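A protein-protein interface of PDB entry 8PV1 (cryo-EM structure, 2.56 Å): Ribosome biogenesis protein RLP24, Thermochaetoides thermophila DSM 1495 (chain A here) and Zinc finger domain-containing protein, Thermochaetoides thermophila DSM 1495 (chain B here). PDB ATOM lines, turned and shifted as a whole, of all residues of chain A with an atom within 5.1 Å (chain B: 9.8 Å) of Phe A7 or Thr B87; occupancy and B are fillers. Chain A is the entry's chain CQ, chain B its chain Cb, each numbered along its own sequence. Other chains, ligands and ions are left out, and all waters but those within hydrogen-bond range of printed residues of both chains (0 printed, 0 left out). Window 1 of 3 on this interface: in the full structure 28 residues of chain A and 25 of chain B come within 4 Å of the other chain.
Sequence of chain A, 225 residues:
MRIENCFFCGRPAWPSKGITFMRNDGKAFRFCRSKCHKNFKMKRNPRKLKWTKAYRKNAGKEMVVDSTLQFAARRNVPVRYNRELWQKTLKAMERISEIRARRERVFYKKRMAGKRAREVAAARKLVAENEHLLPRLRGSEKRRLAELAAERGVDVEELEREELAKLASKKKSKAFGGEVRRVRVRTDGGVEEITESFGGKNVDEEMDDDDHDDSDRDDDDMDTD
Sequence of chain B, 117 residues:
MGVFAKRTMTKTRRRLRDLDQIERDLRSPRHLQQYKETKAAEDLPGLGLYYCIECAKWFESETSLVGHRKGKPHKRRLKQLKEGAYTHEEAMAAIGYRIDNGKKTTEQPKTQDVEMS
O of Phe A7 is in hydrogen-bond range of OH of Tyr B86.
The backbone carbonyl oxygen (O) of Gly A10 lies close to the side-chain amide oxygen (OD1) of Asn A5. The side-chain sulfur of Cys A6 lies close to the backbone NH of Phe A8 (3.4 Å). The backbone NH (N) of Phe A7 lies within hydrogen-bond range of the backbone carbonyl oxygen (O) of Arg A30, at 2.7 Å. The side-chain hydroxyl of Thr B87 sits at hydrogen-bond distance from the side-chain carboxylate of Glu B89, 3.2 Å away.
Among the printed residues, pairs that only touch across the chains: Asn A5 with Ile B95 (3.5 Å), Phe A7 with Thr B87 (3.7 Å), Phe A7 with His B88 (3.4 Å), Phe A7 with Ala B91 (3.9 Å), Phe A8 with Tyr B86 (3.98 Å), Gly A10 with Ile B95 (3.8 Å) and Phe A29 with His B88 (3.5 Å).
Of the printed residues of chain B, Asn A5 touches Ile B95. No residue of chain B comes within 4 Å of Cys A6. Printed residues of chain B within 4 Å of Phe A29: His B88. Printed residues of chain A within 4 Å of Thr B87: Phe A7. The nearest printed residue of chain A that does not touch Thr B87 is Phe A29 (6.2 Å).
Of the 21 printed residues of chain B, 5 touch a printed residue of chain A. Hydrophobic or aromatic side chains of chain B within 4 Å of the printed part of chain A: Tyr B86, His B88, Ala B91 and Ile B95. Hydrophobic or aromatic side chains of chain A that line the printed part of chain B: Phe A7 and Phe A29. Among the printed residues, 8 pairs touch across the chains.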
ATOM      1  N   ASN A   5     -19.369  18.861 -18.449  1.00  0.00           N
ATOM      2  CA  ASN A   5     -19.063  18.074 -17.270  1.00  0.00           C
ATOM      3  C   ASN A   5     -18.302  16.840 -17.714  1.00  0.00           C
ATOM      4  O   ASN A   5     -18.524  16.321 -18.811  1.00  0.00           O
ATOM      5  CB  ASN A   5     -20.329  17.692 -16.501  1.00  0.00           C
ATOM      6  CG  ASN A   5     -20.928  18.867 -15.760  1.00  0.00           C
ATOM      7  OD1 ASN A   5     -20.671  19.062 -14.573  1.00  0.00           O
ATOM      8  ND2 ASN A   5     -21.718  19.669 -16.463  1.00  0.00           N
ATOM      9  N   CYS A   6     -17.372  16.404 -16.871  1.00  0.00           N
ATOM     10  CA  CYS A   6     -16.621  15.193 -17.155  1.00  0.00           C
ATOM     11  C   CYS A   6     -17.560  13.997 -17.157  1.00  0.00           C
ATOM     12  O   CYS A   6     -18.431  13.872 -16.294  1.00  0.00           O
ATOM     13  CB  CYS A   6     -15.512  14.996 -16.124  1.00  0.00           C
ATOM     14  SG  CYS A   6     -14.553  13.484 -16.338  1.00  0.00           S
ATOM     15  N   PHE A   7     -17.403  13.136 -18.162  1.00  0.00           N
ATOM     16  CA  PHE A   7     -18.220  11.931 -18.230  1.00  0.00           C
ATOM     17  C   PHE A   7     -17.929  11.007 -17.057  1.00  0.00           C
ATOM     18  O   PHE A   7     -18.849  10.426 -16.474  1.00  0.00           O
ATOM     19  CB  PHE A   7     -17.980  11.210 -19.557  1.00  0.00           C
ATOM     20  CG  PHE A   7     -18.569   9.829 -19.614  1.00  0.00           C
ATOM     21  CD1 PHE A   7     -19.929   9.651 -19.793  1.00  0.00           C
ATOM     22  CD2 PHE A   7     -17.760   8.708 -19.494  1.00  0.00           C
ATOM     23  CE1 PHE A   7     -20.473   8.385 -19.842  1.00  0.00           C
ATOM     24  CE2 PHE A   7     -18.300   7.442 -19.540  1.00  0.00           C
ATOM     25  CZ  PHE A   7     -19.658   7.281 -19.719  1.00  0.00           C
ATOM     26  N   PHE A   8     -16.659  10.885 -16.681  1.00  0.00           N
ATOM     27  CA  PHE A   8     -16.261   9.901 -15.685  1.00  0.00           C
ATOM     28  C   PHE A   8     -16.532  10.383 -14.263  1.00  0.00           C
ATOM     29  O   PHE A   8     -17.127   9.659 -13.460  1.00  0.00           O
ATOM     30  CB  PHE A   8     -14.784   9.564 -15.866  1.00  0.00           C
ATOM     31  CG  PHE A   8     -14.392   8.235 -15.310  1.00  0.00           C
ATOM     32  CD1 PHE A   8     -13.997   8.114 -13.990  1.00  0.00           C
ATOM     33  CD2 PHE A   8     -14.409   7.105 -16.107  1.00  0.00           C
ATOM     34  CE1 PHE A   8     -13.636   6.893 -13.475  1.00  0.00           C
ATOM     35  CE2 PHE A   8     -14.043   5.878 -15.598  1.00  0.00           C
ATOM     36  CZ  PHE A   8     -13.661   5.772 -14.279  1.00  0.00           C
ATOM     37  N   CYS A   9     -16.103  11.598 -13.930  1.00  0.00           N
ATOM     38  CA  CYS A   9     -16.145  12.062 -12.551  1.00  0.00           C
ATOM     39  C   CYS A   9     -17.119  13.206 -12.302  1.00  0.00           C
ATOM     40  O   CYS A   9     -17.441  13.472 -11.140  1.00  0.00           O
ATOM     41  CB  CYS A   9     -14.741  12.484 -12.094  1.00  0.00           C
ATOM     42  SG  CYS A   9     -14.275  14.144 -12.587  1.00  0.00           S
ATOM     43  N   GLY A  10     -17.589  13.891 -13.341  1.00  0.00           N
ATOM     44  CA  GLY A  10     -18.592  14.921 -13.182  1.00  0.00           C
ATOM     45  C   GLY A  10     -18.075  16.307 -12.860  1.00  0.00           C
ATOM     46  O   GLY A  10     -18.888  17.213 -12.650  1.00  0.00           O
ATOM     47  N   PHE A  29     -17.162  11.128 -25.619  1.00  0.00           N
ATOM     48  CA  PHE A  29     -16.938  11.075 -24.177  1.00  0.00           C
ATOM     49  C   PHE A  29     -15.942  12.164 -23.812  1.00  0.00           C
ATOM     50  O   PHE A  29     -14.792  12.122 -24.252  1.00  0.00           O
ATOM     51  CB  PHE A  29     -16.403   9.711 -23.731  1.00  0.00           C
ATOM     52  CG  PHE A  29     -17.339   8.566 -23.972  1.00  0.00           C
ATOM     53  CD1 PHE A  29     -17.357   7.912 -25.192  1.00  0.00           C
ATOM     54  CD2 PHE A  29     -18.202   8.140 -22.979  1.00  0.00           C
ATOM     55  CE1 PHE A  29     -18.203   6.846 -25.407  1.00  0.00           C
ATOM     56  CE2 PHE A  29     -19.062   7.082 -23.195  1.00  0.00           C
ATOM     57  CZ  PHE A  29     -19.068   6.439 -24.413  1.00  0.00           C
ATOM     58  N   ARG A  30     -16.365  13.121 -22.997  1.00  0.00           N
ATOM     59  CA  ARG A  30     -15.484  14.201 -22.580  1.00  0.00           C
ATOM     60  C   ARG A  30     -14.939  13.922 -21.185  1.00  0.00           C
ATOM     61  O   ARG A  30     -15.705  13.726 -20.239  1.00  0.00           O
ATOM     62  CB  ARG A  30     -16.222  15.537 -22.602  1.00  0.00           C
ATOM     63  CG  ARG A  30     -15.451  16.672 -21.966  1.00  0.00           C
ATOM     64  CD  ARG A  30     -14.279  17.095 -22.840  1.00  0.00           C
ATOM     65  NE  ARG A  30     -13.558  18.230 -22.277  1.00  0.00           N
ATOM     66  CZ  ARG A  30     -13.947  19.492 -22.393  1.00  0.00           C
ATOM     67  NH1 ARG A  30     -15.038  19.820 -23.064  1.00  0.00           N
ATOM     68  NH2 ARG A  30     -13.225  20.450 -21.821  1.00  0.00           N
ATOM     69  N   PHE A  31     -13.617  13.923 -21.063  1.00  0.00           N
ATOM     70  CA  PHE A  31     -12.931  13.738 -19.798  1.00  0.00           C
ATOM     71  C   PHE A  31     -12.214  15.027 -19.433  1.00  0.00           C
ATOM     72  O   PHE A  31     -11.582  15.661 -20.281  1.00  0.00           O
ATOM     73  CB  PHE A  31     -11.923  12.590 -19.880  1.00  0.00           C
ATOM     74  CG  PHE A  31     -12.486  11.344 -20.477  1.00  0.00           C
ATOM     75  CD1 PHE A  31     -13.337  10.537 -19.747  1.00  0.00           C
ATOM     76  CD2 PHE A  31     -12.186  10.991 -21.780  1.00  0.00           C
ATOM     77  CE1 PHE A  31     -13.867   9.399 -20.300  1.00  0.00           C
ATOM     78  CE2 PHE A  31     -12.714   9.853 -22.338  1.00  0.00           C
ATOM     79  CZ  PHE A  31     -13.556   9.058 -21.596  1.00  0.00           C
ATOM     80  N   PHE A  40     -11.032   5.359 -17.667  1.00  0.00           N
ATOM     81  CA  PHE A  40     -11.965   4.924 -18.702  1.00  0.00           C
ATOM     82  C   PHE A  40     -11.318   3.915 -19.647  1.00  0.00           C
ATOM     83  O   PHE A  40     -11.951   2.924 -20.030  1.00  0.00           O
ATOM     84  CB  PHE A  40     -12.480   6.136 -19.479  1.00  0.00           C
ATOM     85  CG  PHE A  40     -13.463   5.794 -20.565  1.00  0.00           C
ATOM     86  CD1 PHE A  40     -14.804   5.639 -20.269  1.00  0.00           C
ATOM     87  CD2 PHE A  40     -13.050   5.646 -21.881  1.00  0.00           C
ATOM     88  CE1 PHE A  40     -15.713   5.330 -21.257  1.00  0.00           C
ATOM     89  CE2 PHE A  40     -13.954   5.334 -22.871  1.00  0.00           C
ATOM     90  CZ  PHE A  40     -15.288   5.178 -22.558  1.00  0.00           C
ATOM     91  N   ASP B  18     -17.064  -2.109 -25.340  1.00  0.00           N
ATOM     92  CA  ASP B  18     -17.510  -1.580 -24.060  1.00  0.00           C
ATOM     93  C   ASP B  18     -18.781  -2.262 -23.564  1.00  0.00           C
ATOM     94  O   ASP B  18     -19.547  -2.861 -24.330  1.00  0.00           O
ATOM     95  CB  ASP B  18     -17.746  -0.074 -24.146  1.00  0.00           C
ATOM     96  CG  ASP B  18     -16.490   0.729 -23.890  1.00  0.00           C
ATOM     97  OD1 ASP B  18     -15.803   0.451 -22.887  1.00  0.00           O
ATOM     98  OD2 ASP B  18     -16.197   1.651 -24.679  1.00  0.00           O
ATOM     99  N   LEU B  19     -19.011  -2.127 -22.256  1.00  0.00           N
ATOM    100  CA  LEU B  19     -20.102  -2.838 -21.599  1.00  0.00           C
ATOM    101  C   LEU B  19     -21.462  -2.264 -21.977  1.00  0.00           C
ATOM    102  O   LEU B  19     -22.447  -3.004 -22.062  1.00  0.00           O
ATOM    103  CB  LEU B  19     -19.904  -2.801 -20.086  1.00  0.00           C
ATOM    104  CG  LEU B  19     -20.704  -3.816 -19.270  1.00  0.00           C
ATOM    105  CD1 LEU B  19     -20.278  -5.224 -19.619  1.00  0.00           C
ATOM    106  CD2 LEU B  19     -20.524  -3.555 -17.791  1.00  0.00           C
ATOM    107  N   ASP B  20     -21.547  -0.947 -22.188  1.00  0.00           N
ATOM    108  CA  ASP B  20     -22.818  -0.367 -22.616  1.00  0.00           C
ATOM    109  C   ASP B  20     -23.170  -0.810 -24.032  1.00  0.00           C
ATOM    110  O   ASP B  20     -24.346  -1.052 -24.342  1.00  0.00           O
ATOM    111  CB  ASP B  20     -22.773   1.158 -22.503  1.00  0.00           C
ATOM    112  CG  ASP B  20     -21.785   1.786 -23.457  1.00  0.00           C
ATOM    113  OD1 ASP B  20     -22.061   2.893 -23.964  1.00  0.00           O
ATOM    114  OD2 ASP B  20     -20.726   1.176 -23.697  1.00  0.00           O
ATOM    115  N   GLN B  21     -22.158  -0.958 -24.889  1.00  0.00           N
ATOM    116  CA  GLN B  21     -22.368  -1.568 -26.195  1.00  0.00           C
ATOM    117  C   GLN B  21     -22.821  -3.011 -26.056  1.00  0.00           C
ATOM    118  O   GLN B  21     -23.652  -3.481 -26.840  1.00  0.00           O
ATOM    119  CB  GLN B  21     -21.091  -1.488 -27.028  1.00  0.00           C
ATOM    120  CG  GLN B  21     -20.522  -0.094 -27.162  1.00  0.00           C
ATOM    121  CD  GLN B  21     -19.313  -0.050 -28.068  1.00  0.00           C
ATOM    122  OE1 GLN B  21     -18.255  -0.580 -27.737  1.00  0.00           O
ATOM    123  NE2 GLN B  21     -19.464   0.584 -29.221  1.00  0.00           N
ATOM    124  N   ILE B  22     -22.291  -3.728 -25.061  1.00  0.00           N
ATOM    125  CA  ILE B  22     -22.721  -5.106 -24.822  1.00  0.00           C
ATOM    126  C   ILE B  22     -24.191  -5.158 -24.405  1.00  0.00           C
ATOM    127  O   ILE B  22     -24.950  -6.009 -24.889  1.00  0.00           O
ATOM    128  CB  ILE B  22     -21.797  -5.779 -23.787  1.00  0.00           C
ATOM    129  CG1 ILE B  22     -20.418  -6.026 -24.399  1.00  0.00           C
ATOM    130  CG2 ILE B  22     -22.382  -7.088 -23.282  1.00  0.00           C
ATOM    131  CD1 ILE B  22     -19.341  -6.281 -23.388  1.00  0.00           C
ATOM    132  N   GLU B  23     -24.622  -4.251 -23.518  1.00  0.00           N
ATOM    133  CA  GLU B  23     -26.040  -4.224 -23.142  1.00  0.00           C
ATOM    134  C   GLU B  23     -26.922  -3.872 -24.327  1.00  0.00           C
ATOM    135  O   GLU B  23     -28.029  -4.402 -24.464  1.00  0.00           O
ATOM    136  CB  GLU B  23     -26.362  -3.243 -22.012  1.00  0.00           C
ATOM    137  CG  GLU B  23     -25.425  -3.054 -20.871  1.00  0.00           C
ATOM    138  CD  GLU B  23     -26.111  -2.250 -19.789  1.00  0.00           C
ATOM    139  OE1 GLU B  23     -27.321  -2.470 -19.583  1.00  0.00           O
ATOM    140  OE2 GLU B  23     -25.480  -1.389 -19.159  1.00  0.00           O
ATOM    141  N   ARG B  24     -26.472  -2.945 -25.172  1.00  0.00           N
ATOM    142  CA  ARG B  24     -27.289  -2.566 -26.319  1.00  0.00           C
ATOM    143  C   ARG B  24     -27.361  -3.701 -27.339  1.00  0.00           C
ATOM    144  O   ARG B  24     -28.395  -3.893 -27.991  1.00  0.00           O
ATOM    145  CB  ARG B  24     -26.746  -1.278 -26.934  1.00  0.00           C
ATOM    146  CG  ARG B  24     -27.579  -0.716 -28.066  1.00  0.00           C
ATOM    147  CD  ARG B  24     -26.983   0.580 -28.579  1.00  0.00           C
ATOM    148  NE  ARG B  24     -27.011   1.621 -27.557  1.00  0.00           N
ATOM    149  CZ  ARG B  24     -25.936   2.139 -26.978  1.00  0.00           C
ATOM    150  NH1 ARG B  24     -24.716   1.747 -27.308  1.00  0.00           N
ATOM    151  NH2 ARG B  24     -26.088   3.073 -26.045  1.00  0.00           N
ATOM    152  N   ARG B  27     -29.913  -6.077 -25.821  1.00  0.00           N
ATOM    153  CA  ARG B  27     -31.272  -5.553 -25.880  1.00  0.00           C
ATOM    154  C   ARG B  27     -31.819  -5.544 -27.303  1.00  0.00           C
ATOM    155  O   ARG B  27     -32.987  -5.884 -27.520  1.00  0.00           O
ATOM    156  CB  ARG B  27     -31.306  -4.143 -25.287  1.00  0.00           C
ATOM    157  CG  ARG B  27     -32.695  -3.547 -25.177  1.00  0.00           C
ATOM    158  CD  ARG B  27     -32.666  -2.175 -24.518  1.00  0.00           C
ATOM    159  NE  ARG B  27     -31.945  -1.197 -25.322  1.00  0.00           N
ATOM    160  CZ  ARG B  27     -30.801  -0.629 -24.967  1.00  0.00           C
ATOM    161  NH1 ARG B  27     -30.219  -0.909 -23.813  1.00  0.00           N
ATOM    162  NH2 ARG B  27     -30.229   0.246 -25.788  1.00  0.00           N
ATOM    163  N   GLU B  83     -25.241  -5.369 -12.601  1.00  0.00           N
ATOM    164  CA  GLU B  83     -25.116  -4.051 -11.985  1.00  0.00           C
ATOM    165  C   GLU B  83     -25.502  -2.936 -12.950  1.00  0.00           C
ATOM    166  O   GLU B  83     -26.049  -1.913 -12.523  1.00  0.00           O
ATOM    167  CB  GLU B  83     -23.691  -3.834 -11.479  1.00  0.00           C
ATOM    168  CG  GLU B  83     -23.374  -4.555 -10.186  1.00  0.00           C
ATOM    169  CD  GLU B  83     -21.925  -4.401  -9.778  1.00  0.00           C
ATOM    170  OE1 GLU B  83     -21.067  -4.233 -10.669  1.00  0.00           O
ATOM    171  OE2 GLU B  83     -21.645  -4.435  -8.561  1.00  0.00           O
ATOM    172  N   GLY B  84     -25.229  -3.111 -14.241  1.00  0.00           N
ATOM    173  CA  GLY B  84     -25.531  -2.102 -15.237  1.00  0.00           C
ATOM    174  C   GLY B  84     -24.322  -1.253 -15.570  1.00  0.00           C
ATOM    175  O   GLY B  84     -23.614  -0.805 -14.664  1.00  0.00           O
ATOM    176  N   ALA B  85     -24.065  -1.025 -16.855  1.00  0.00           N
ATOM    177  CA  ALA B  85     -22.915  -0.216 -17.234  1.00  0.00           C
ATOM    178  C   ALA B  85     -23.223   1.268 -17.090  1.00  0.00           C
ATOM    179  O   ALA B  85     -24.376   1.683 -16.945  1.00  0.00           O
ATOM    180  CB  ALA B  85     -22.472  -0.515 -18.665  1.00  0.00           C
ATOM    181  N   TYR B  86     -22.165   2.067 -17.132  1.00  0.00           N
ATOM    182  CA  TYR B  86     -22.260   3.499 -16.906  1.00  0.00           C
ATOM    183  C   TYR B  86     -22.466   4.239 -18.221  1.00  0.00           C
ATOM    184  O   TYR B  86     -21.696   4.074 -19.169  1.00  0.00           O
ATOM    185  CB  TYR B  86     -20.988   3.978 -16.213  1.00  0.00           C
ATOM    186  CG  TYR B  86     -20.991   5.413 -15.778  1.00  0.00           C
ATOM    187  CD1 TYR B  86     -21.714   5.824 -14.673  1.00  0.00           C
ATOM    188  CD2 TYR B  86     -20.240   6.356 -16.457  1.00  0.00           C
ATOM    189  CE1 TYR B  86     -21.707   7.134 -14.272  1.00  0.00           C
ATOM    190  CE2 TYR B  86     -20.221   7.667 -16.059  1.00  0.00           C
ATOM    191  CZ  TYR B  86     -20.954   8.054 -14.964  1.00  0.00           C
ATOM    192  OH  TYR B  86     -20.937   9.365 -14.562  1.00  0.00           O
ATOM    193  N   THR B  87     -23.504   5.070 -18.268  1.00  0.00           N
ATOM    194  CA  THR B  87     -23.904   5.771 -19.481  1.00  0.00           C
ATOM    195  C   THR B  87     -23.962   7.273 -19.226  1.00  0.00           C
ATOM    196  O   THR B  87     -23.751   7.753 -18.108  1.00  0.00           O
ATOM    197  CB  THR B  87     -25.258   5.263 -19.991  1.00  0.00           C
ATOM    198  OG1 THR B  87     -26.224   5.331 -18.936  1.00  0.00           O
ATOM    199  CG2 THR B  87     -25.146   3.834 -20.486  1.00  0.00           C
ATOM    200  N   HIS B  88     -24.258   8.020 -20.294  1.00  0.00           N
ATOM    201  CA  HIS B  88     -24.393   9.469 -20.183  1.00  0.00           C
ATOM    202  C   HIS B  88     -25.648   9.864 -19.418  1.00  0.00           C
ATOM    203  O   HIS B  88     -25.673  10.924 -18.786  1.00  0.00           O
ATOM    204  CB  HIS B  88     -24.389  10.110 -21.573  1.00  0.00           C
ATOM    205  CG  HIS B  88     -23.019  10.363 -22.121  1.00  0.00           C
ATOM    206  ND1 HIS B  88     -22.359   9.464 -22.932  1.00  0.00           N
ATOM    207  CD2 HIS B  88     -22.185  11.419 -21.977  1.00  0.00           C
ATOM    208  CE1 HIS B  88     -21.178   9.955 -23.259  1.00  0.00           C
ATOM    209  NE2 HIS B  88     -21.048  11.141 -22.694  1.00  0.00           N
ATOM    210  N   GLU B  89     -26.696   9.035 -19.460  1.00  0.00           N
ATOM    211  CA  GLU B  89     -27.881   9.296 -18.648  1.00  0.00           C
ATOM    212  C   GLU B  89     -27.560   9.195 -17.162  1.00  0.00           C
ATOM    213  O   GLU B  89     -27.965  10.056 -16.370  1.00  0.00           O
ATOM    214  CB  GLU B  89     -29.003   8.324 -19.022  1.00  0.00           C
ATOM    215  CG  GLU B  89     -29.565   8.513 -20.428  1.00  0.00           C
ATOM    216  CD  GLU B  89     -28.735   7.828 -21.500  1.00  0.00           C
ATOM    217  OE1 GLU B  89     -27.752   7.145 -21.150  1.00  0.00           O
ATOM    218  OE2 GLU B  89     -29.056   7.986 -22.695  1.00  0.00           O
ATOM    219  N   GLU B  90     -26.811   8.160 -16.774  1.00  0.00           N
ATOM    220  CA  GLU B  90     -26.359   8.039 -15.394  1.00  0.00           C
ATOM    221  C   GLU B  90     -25.395   9.162 -15.033  1.00  0.00           C
ATOM    222  O   GLU B  90     -25.408   9.657 -13.901  1.00  0.00           O
ATOM    223  CB  GLU B  90     -25.714   6.670 -15.177  1.00  0.00           C
ATOM    224  CG  GLU B  90     -25.196   6.427 -13.772  1.00  0.00           C
ATOM    225  CD  GLU B  90     -24.834   4.979 -13.529  1.00  0.00           C
ATOM    226  OE1 GLU B  90     -25.028   4.156 -14.446  1.00  0.00           O
ATOM    227  OE2 GLU B  90     -24.346   4.663 -12.425  1.00  0.00           O
ATOM    228  N   ALA B  91     -24.573   9.594 -15.995  1.00  0.00           N
ATOM    229  CA  ALA B  91     -23.659  10.709 -15.756  1.00  0.00           C
ATOM    230  C   ALA B  91     -24.411  12.010 -15.489  1.00  0.00           C
ATOM    231  O   ALA B  91     -24.022  12.787 -14.611  1.00  0.00           O
ATOM    232  CB  ALA B  91     -22.712  10.869 -16.944  1.00  0.00           C
ATOM    233  N   MET B  92     -25.485  12.266 -16.241  1.00  0.00           N
ATOM    234  CA  MET B  92     -26.293  13.457 -15.994  1.00  0.00           C
ATOM    235  C   MET B  92     -27.054  13.353 -14.678  1.00  0.00           C
ATOM    236  O   MET B  92     -27.207  14.350 -13.962  1.00  0.00           O
ATOM    237  CB  MET B  92     -27.265  13.696 -17.148  1.00  0.00           C
ATOM    238  CG  MET B  92     -26.607  14.060 -18.458  1.00  0.00           C
ATOM    239  SD  MET B  92     -27.829  14.385 -19.738  1.00  0.00           S
ATOM    240  CE  MET B  92     -28.381  12.722 -20.095  1.00  0.00           C
ATOM    241  N   ALA B  93     -27.550  12.158 -14.347  1.00  0.00           N
ATOM    242  CA  ALA B  93     -28.250  11.987 -13.079  1.00  0.00           C
ATOM    243  C   ALA B  93     -27.304  12.112 -11.889  1.00  0.00           C
ATOM    244  O   ALA B  93     -27.742  12.458 -10.787  1.00  0.00           O
ATOM    245  CB  ALA B  93     -28.968  10.639 -13.052  1.00  0.00           C
ATOM    246  N   ALA B  94     -26.013  11.833 -12.090  1.00  0.00           N
ATOM    247  CA  ALA B  94     -25.048  11.963 -11.004  1.00  0.00           C
ATOM    248  C   ALA B  94     -24.817  13.417 -10.617  1.00  0.00           C
ATOM    249  O   ALA B  94     -24.507  13.706  -9.457  1.00  0.00           O
ATOM    250  CB  ALA B  94     -23.728  11.301 -11.396  1.00  0.00           C
ATOM    251  N   ILE B  95     -24.955  14.341 -11.566  1.00  0.00           N
ATOM    252  CA  ILE B  95     -24.782  15.765 -11.310  1.00  0.00           C
ATOM    253  C   ILE B  95     -26.117  16.490 -11.221  1.00  0.00           C
ATOM    254  O   ILE B  95     -26.145  17.700 -10.984  1.00  0.00           O
ATOM    255  CB  ILE B  95     -23.881  16.418 -12.369  1.00  0.00           C
ATOM    256  CG1 ILE B  95     -24.430  16.141 -13.768  1.00  0.00           C
ATOM    257  CG2 ILE B  95     -22.453  15.917 -12.237  1.00  0.00           C
ATOM    258  CD1 ILE B  95     -23.640  16.780 -14.874  1.00  0.00           C
